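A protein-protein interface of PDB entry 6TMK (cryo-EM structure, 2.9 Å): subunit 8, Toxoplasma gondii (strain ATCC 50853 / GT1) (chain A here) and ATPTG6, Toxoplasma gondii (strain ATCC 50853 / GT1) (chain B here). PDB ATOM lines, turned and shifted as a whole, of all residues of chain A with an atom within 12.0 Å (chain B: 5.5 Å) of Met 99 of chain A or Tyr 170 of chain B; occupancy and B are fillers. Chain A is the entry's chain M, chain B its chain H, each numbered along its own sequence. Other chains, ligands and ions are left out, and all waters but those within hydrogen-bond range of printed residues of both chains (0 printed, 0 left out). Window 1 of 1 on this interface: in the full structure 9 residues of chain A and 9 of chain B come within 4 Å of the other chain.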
ATOM      1  N   ALA A  96     -10.414  -4.129 -28.685  1.00  0.00           N
ATOM      2  CA  ALA A  96      -9.133  -3.721 -28.120  1.00  0.00           C
ATOM      3  C   ALA A  96      -8.468  -2.678 -29.005  1.00  0.00           C
ATOM      4  O   ALA A  96      -8.894  -2.450 -30.137  1.00  0.00           O
ATOM      5  CB  ALA A  96      -8.231  -4.915 -27.953  1.00  0.00           C
ATOM      6  N   SER A  97      -7.426  -2.048 -28.488  1.00  0.00           N
ATOM      7  CA  SER A  97      -6.752  -0.978 -29.197  1.00  0.00           C
ATOM      8  C   SER A  97      -5.472  -1.491 -29.832  1.00  0.00           C
ATOM      9  O   SER A  97      -4.924  -2.514 -29.414  1.00  0.00           O
ATOM     10  CB  SER A  97      -6.422   0.174 -28.244  1.00  0.00           C
ATOM     11  OG  SER A  97      -5.478  -0.218 -27.271  1.00  0.00           O
ATOM     12  N   PRO A  98      -4.958  -0.798 -30.848  1.00  0.00           N
ATOM     13  CA  PRO A  98      -3.780  -1.319 -31.548  1.00  0.00           C
ATOM     14  C   PRO A  98      -2.492  -1.191 -30.756  1.00  0.00           C
ATOM     15  O   PRO A  98      -1.505  -1.840 -31.114  1.00  0.00           O
ATOM     16  CB  PRO A  98      -3.738  -0.484 -32.834  1.00  0.00           C
ATOM     17  CG  PRO A  98      -4.570   0.691 -32.576  1.00  0.00           C
ATOM     18  CD  PRO A  98      -5.589   0.306 -31.576  1.00  0.00           C
ATOM     19  N   MET A  99      -2.458  -0.378 -29.703  1.00  0.00           N
ATOM     20  CA  MET A  99      -1.235  -0.173 -28.942  1.00  0.00           C
ATOM     21  C   MET A  99      -1.027  -1.187 -27.826  1.00  0.00           C
ATOM     22  O   MET A  99       0.081  -1.261 -27.284  1.00  0.00           O
ATOM     23  CB  MET A  99      -1.203   1.244 -28.377  1.00  0.00           C
ATOM     24  CG  MET A  99      -0.538   2.247 -29.307  1.00  0.00           C
ATOM     25  SD  MET A  99      -1.278   2.424 -30.935  1.00  0.00           S
ATOM     26  CE  MET A  99      -2.746   3.327 -30.522  1.00  0.00           C
ATOM     27  N   LEU A 100      -2.048  -1.957 -27.458  1.00  0.00           N
ATOM     28  CA  LEU A 100      -1.826  -3.089 -26.567  1.00  0.00           C
ATOM     29  C   LEU A 100      -1.018  -4.185 -27.240  1.00  0.00           C
ATOM     30  O   LEU A 100      -0.454  -5.040 -26.550  1.00  0.00           O
ATOM     31  CB  LEU A 100      -3.153  -3.640 -26.061  1.00  0.00           C
ATOM     32  CG  LEU A 100      -3.989  -2.643 -25.260  1.00  0.00           C
ATOM     33  CD1 LEU A 100      -5.340  -3.225 -24.929  1.00  0.00           C
ATOM     34  CD2 LEU A 100      -3.269  -2.229 -23.991  1.00  0.00           C
ATOM     35  N   PHE A 101      -0.963  -4.180 -28.568  1.00  0.00           N
ATOM     36  CA  PHE A 101      -0.120  -5.099 -29.314  1.00  0.00           C
ATOM     37  C   PHE A 101       1.330  -4.647 -29.257  1.00  0.00           C
ATOM     38  O   PHE A 101       1.634  -3.469 -29.463  1.00  0.00           O
ATOM     39  CB  PHE A 101      -0.599  -5.191 -30.759  1.00  0.00           C
ATOM     40  CG  PHE A 101       0.020  -6.308 -31.525  1.00  0.00           C
ATOM     41  CD1 PHE A 101      -0.519  -7.574 -31.470  1.00  0.00           C
ATOM     42  CD2 PHE A 101       1.133  -6.095 -32.304  1.00  0.00           C
ATOM     43  CE1 PHE A 101       0.043  -8.600 -32.168  1.00  0.00           C
ATOM     44  CE2 PHE A 101       1.697  -7.122 -33.006  1.00  0.00           C
ATOM     45  CZ  PHE A 101       1.151  -8.376 -32.941  1.00  0.00           C
ATOM     46  N   THR A 102       2.226  -5.594 -28.982  1.00  0.00           N
ATOM     47  CA  THR A 102       3.646  -5.296 -28.869  1.00  0.00           C
ATOM     48  C   THR A 102       4.486  -6.206 -29.758  1.00  0.00           C
ATOM     49  O   THR A 102       5.555  -5.802 -30.225  1.00  0.00           O
ATOM     50  CB  THR A 102       4.087  -5.428 -27.408  1.00  0.00           C
ATOM     51  OG1 THR A 102       5.480  -5.117 -27.293  1.00  0.00           O
ATOM     52  CG2 THR A 102       3.848  -6.841 -26.901  1.00  0.00           C
ATOM     53  N   ASP A 103       4.015  -7.429 -30.005  1.00  0.00           N
ATOM     54  CA  ASP A 103       4.820  -8.445 -30.685  1.00  0.00           C
ATOM     55  C   ASP A 103       4.848  -8.162 -32.187  1.00  0.00           C
ATOM     56  O   ASP A 103       4.253  -8.861 -33.010  1.00  0.00           O
ATOM     57  CB  ASP A 103       4.277  -9.837 -30.387  1.00  0.00           C
ATOM     58  CG  ASP A 103       5.375 -10.875 -30.204  1.00  0.00           C
ATOM     59  OD1 ASP A 103       6.562 -10.541 -30.401  1.00  0.00           O
ATOM     60  OD2 ASP A 103       5.050 -12.031 -29.864  1.00  0.00           O
ATOM     61  N   TYR A 104       5.585  -7.111 -32.539  1.00  0.00           N
ATOM     62  CA  TYR A 104       5.682  -6.650 -33.916  1.00  0.00           C
ATOM     63  C   TYR A 104       6.879  -7.225 -34.657  1.00  0.00           C
ATOM     64  O   TYR A 104       6.915  -7.162 -35.891  1.00  0.00           O
ATOM     65  CB  TYR A 104       5.763  -5.126 -33.973  1.00  0.00           C
ATOM     66  CG  TYR A 104       4.436  -4.426 -34.127  1.00  0.00           C
ATOM     67  CD1 TYR A 104       3.641  -4.643 -35.240  1.00  0.00           C
ATOM     68  CD2 TYR A 104       3.991  -3.529 -33.175  1.00  0.00           C
ATOM     69  CE1 TYR A 104       2.436  -4.004 -35.388  1.00  0.00           C
ATOM     70  CE2 TYR A 104       2.790  -2.882 -33.315  1.00  0.00           C
ATOM     71  CZ  TYR A 104       2.014  -3.117 -34.424  1.00  0.00           C
ATOM     72  OH  TYR A 104       0.810  -2.468 -34.561  1.00  0.00           O
ATOM     73  N   ALA B 167      -7.587   9.358 -37.782  1.00  0.00           N
ATOM     74  CA  ALA B 167      -6.516   8.397 -37.590  1.00  0.00           C
ATOM     75  C   ALA B 167      -5.713   8.638 -36.319  1.00  0.00           C
ATOM     76  O   ALA B 167      -5.092   7.698 -35.813  1.00  0.00           O
ATOM     77  CB  ALA B 167      -5.591   8.432 -38.803  1.00  0.00           C
ATOM     78  N   CYS B 168      -5.712   9.858 -35.792  1.00  0.00           N
ATOM     79  CA  CYS B 168      -4.968  10.209 -34.591  1.00  0.00           C
ATOM     80  C   CYS B 168      -5.749   9.921 -33.308  1.00  0.00           C
ATOM     81  O   CYS B 168      -5.291  10.265 -32.209  1.00  0.00           O
ATOM     82  CB  CYS B 168      -4.565  11.677 -34.670  1.00  0.00           C
ATOM     83  SG  CYS B 168      -4.041  12.186 -36.336  1.00  0.00           S
ATOM     84  N   LYS B 169      -6.901   9.269 -33.443  1.00  0.00           N
ATOM     85  CA  LYS B 169      -7.815   9.020 -32.336  1.00  0.00           C
ATOM     86  C   LYS B 169      -7.139   8.250 -31.208  1.00  0.00           C
ATOM     87  O   LYS B 169      -7.050   8.724 -30.065  1.00  0.00           O
ATOM     88  CB  LYS B 169      -9.020   8.259 -32.878  1.00  0.00           C
ATOM     89  CG  LYS B 169      -9.993   7.767 -31.869  1.00  0.00           C
ATOM     90  CD  LYS B 169     -11.311   7.466 -32.524  1.00  0.00           C
ATOM     91  CE  LYS B 169     -11.168   6.338 -33.515  1.00  0.00           C
ATOM     92  NZ  LYS B 169     -12.467   5.767 -33.927  1.00  0.00           N
ATOM     93  N   TYR B 170      -6.685   7.038 -31.508  1.00  0.00           N
ATOM     94  CA  TYR B 170      -6.100   6.190 -30.488  1.00  0.00           C
ATOM     95  C   TYR B 170      -4.795   6.758 -29.956  1.00  0.00           C
ATOM     96  O   TYR B 170      -4.426   6.466 -28.820  1.00  0.00           O
ATOM     97  CB  TYR B 170      -5.887   4.785 -31.042  1.00  0.00           C
ATOM     98  CG  TYR B 170      -7.159   3.987 -31.167  1.00  0.00           C
ATOM     99  CD1 TYR B 170      -7.679   3.300 -30.086  1.00  0.00           C
ATOM    100  CD2 TYR B 170      -7.843   3.923 -32.367  1.00  0.00           C
ATOM    101  CE1 TYR B 170      -8.837   2.574 -30.199  1.00  0.00           C
ATOM    102  CE2 TYR B 170      -9.001   3.203 -32.486  1.00  0.00           C
ATOM    103  CZ  TYR B 170      -9.494   2.530 -31.401  1.00  0.00           C
ATOM    104  OH  TYR B 170     -10.654   1.806 -31.519  1.00  0.00           O
ATOM    105  N   LEU B 171      -4.117   7.604 -30.726  1.00  0.00           N
ATOM    106  CA  LEU B 171      -2.909   8.246 -30.224  1.00  0.00           C
ATOM    107  C   LEU B 171      -3.240   9.279 -29.155  1.00  0.00           C
ATOM    108  O   LEU B 171      -2.563   9.356 -28.116  1.00  0.00           O
ATOM    109  CB  LEU B 171      -2.163   8.895 -31.382  1.00  0.00           C
ATOM    110  CG  LEU B 171      -1.618   7.951 -32.443  1.00  0.00           C
ATOM    111  CD1 LEU B 171      -1.133   8.715 -33.647  1.00  0.00           C
ATOM    112  CD2 LEU B 171      -0.514   7.115 -31.874  1.00  0.00           C
ATOM    113  N   MET B 172      -4.270  10.090 -29.396  1.00  0.00           N
ATOM    114  CA  MET B 172      -4.746  11.000 -28.362  1.00  0.00           C
ATOM    115  C   MET B 172      -5.189  10.231 -27.120  1.00  0.00           C
ATOM    116  O   MET B 172      -4.853  10.605 -25.984  1.00  0.00           O
ATOM    117  CB  MET B 172      -5.875  11.859 -28.929  1.00  0.00           C
ATOM    118  CG  MET B 172      -6.029  13.209 -28.273  1.00  0.00           C
ATOM    119  SD  MET B 172      -6.819  14.435 -29.321  1.00  0.00           S
ATOM    120  CE  MET B 172      -8.215  13.499 -29.897  1.00  0.00           C
ATOM    121  N   ILE B 173      -5.922   9.134 -27.322  1.00  0.00           N
ATOM    122  CA  ILE B 173      -6.358   8.312 -26.196  1.00  0.00           C
ATOM    123  C   ILE B 173      -5.159   7.763 -25.431  1.00  0.00           C
ATOM    124  O   ILE B 173      -5.189   7.655 -24.202  1.00  0.00           O
ATOM    125  CB  ILE B 173      -7.286   7.184 -26.680  1.00  0.00           C
ATOM    126  CG1 ILE B 173      -8.623   7.755 -27.123  1.00  0.00           C
ATOM    127  CG2 ILE B 173      -7.534   6.187 -25.583  1.00  0.00           C
ATOM    128  CD1 ILE B 173      -9.327   6.931 -28.147  1.00  0.00           C
ATOM    129  N   GLU B 174      -4.082   7.423 -26.139  1.00  0.00           N
ATOM    130  CA  GLU B 174      -2.917   6.847 -25.477  1.00  0.00           C
ATOM    131  C   GLU B 174      -2.169   7.886 -24.658  1.00  0.00           C
ATOM    132  O   GLU B 174      -1.672   7.578 -23.573  1.00  0.00           O
ATOM    133  CB  GLU B 174      -1.984   6.199 -26.493  1.00  0.00           C
ATOM    134  CG  GLU B 174      -2.404   4.817 -26.909  1.00  0.00           C
ATOM    135  CD  GLU B 174      -2.240   3.804 -25.792  1.00  0.00           C
ATOM    136  OE1 GLU B 174      -1.241   3.895 -25.047  1.00  0.00           O
ATOM    137  OE2 GLU B 174      -3.113   2.922 -25.652  1.00  0.00           O
ATOM    138  N   GLU B 175      -2.052   9.114 -25.159  1.00  0.00           N
ATOM    139  CA  GLU B 175      -1.389  10.126 -24.342  1.00  0.00           C
ATOM    140  C   GLU B 175      -2.216  10.444 -23.101  1.00  0.00           C
ATOM    141  O   GLU B 175      -1.662  10.612 -22.006  1.00  0.00           O
ATOM    142  CB  GLU B 175      -1.097  11.383 -25.159  1.00  0.00           C
ATOM    143  CG  GLU B 175      -2.277  12.053 -25.779  1.00  0.00           C
ATOM    144  CD  GLU B 175      -1.897  13.372 -26.426  1.00  0.00           C
ATOM    145  OE1 GLU B 175      -1.173  14.154 -25.774  1.00  0.00           O
ATOM    146  OE2 GLU B 175      -2.307  13.623 -27.581  1.00  0.00           O
ATOM    147  N   TRP B 198       3.803  10.331 -27.305  1.00  0.00           N
ATOM    148  CA  TRP B 198       2.512  10.126 -27.938  1.00  0.00           C
ATOM    149  C   TRP B 198       1.961  11.431 -28.463  1.00  0.00           C
ATOM    150  O   TRP B 198       1.276  11.447 -29.493  1.00  0.00           O
ATOM    151  CB  TRP B 198       1.521   9.501 -26.965  1.00  0.00           C
ATOM    152  CG  TRP B 198       1.894   8.148 -26.536  1.00  0.00           C
ATOM    153  CD1 TRP B 198       2.210   7.748 -25.281  1.00  0.00           C
ATOM    154  CD2 TRP B 198       2.009   6.998 -27.366  1.00  0.00           C
ATOM    155  NE1 TRP B 198       2.515   6.416 -25.273  1.00  0.00           N
ATOM    156  CE2 TRP B 198       2.397   5.931 -26.547  1.00  0.00           C
ATOM    157  CE3 TRP B 198       1.822   6.767 -28.729  1.00  0.00           C
ATOM    158  CZ2 TRP B 198       2.599   4.654 -27.040  1.00  0.00           C
ATOM    159  CZ3 TRP B 198       2.023   5.499 -29.212  1.00  0.00           C
ATOM    160  CH2 TRP B 198       2.407   4.460 -28.372  1.00  0.00           C
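Of the printed residues of chain B, Ser 97 of chain A touches Tyr 170.
Printed residues of chain B within 4 Å of Pro 98 of chain A: Tyr 170.
Of chain B, only Tyr 170 (3.5 Å), Glu 174 (3.7 Å) and Trp 198 (3.8 Å) come within 4 Å of Met 99 of chain A.
Asp 103 of chain A touches none of the printed residues of chain B.
No residue of chain A comes within 4 Å of Ala 167 of chain B.
No residue of chain A comes within 4 Å of Cys 168 of chain B.
Of chain A, only Ser 97 (3.8 Å), Pro 98 (3.9 Å) and Met 99 (3.5 Å) come within 4 Å of Tyr 170 of chain B.
No residue of chain A comes within 4 Å of Leu 171 of chain B.
Met 172 of chain B touches none of the printed residues of chain A.
No residue of chain A comes within 4 Å of Ile 173 of chain B.
Of chain A, only Met 99 comes within 4 Å of Glu 174 of chain B.
Glu 175 of chain B touches none of the printed residues of chain A.
Of the printed residues of chain A, Trp 198 of chain B touches Met 99 (3.8 Å).
The nearest printed residue of chain B that does not touch Pro 98 of chain A is Glu 174 of chain B (6.6 Å).
Of the 9 printed residues of chain A, 3 touch a printed residue of chain B.
Printed residues of chain A that touch a printed residue of chain B: Ser 97, Pro 98 and Met 99.
Hydrophobic or aromatic side chains of chain A within 4 Å of the printed part of chain B: Pro 98 and Met 99.
Of the 10 printed residues of chain B, 3 touch a printed residue of chain A.
Printed residues of chain B that touch a printed residue of chain A: Tyr 170, Glu 174 and Trp 198.
Hydrophobic or aromatic side chains of chain B within 4 Å of the printed part of chain A: Tyr 170 and Trp 198.
Among the printed residues, 5 pairs touch across the chains.
Among the printed residues, merely in contact across the chains: Met 99 of chain A with Tyr 170 of chain B, Met 99 of chain A with Glu 174 of chain B, Met 99 of chain A with Trp 198 of chain B, Ser 97 of chain A with Tyr 170 of chain B and Pro 98 of chain A with Tyr 170 of chain B.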
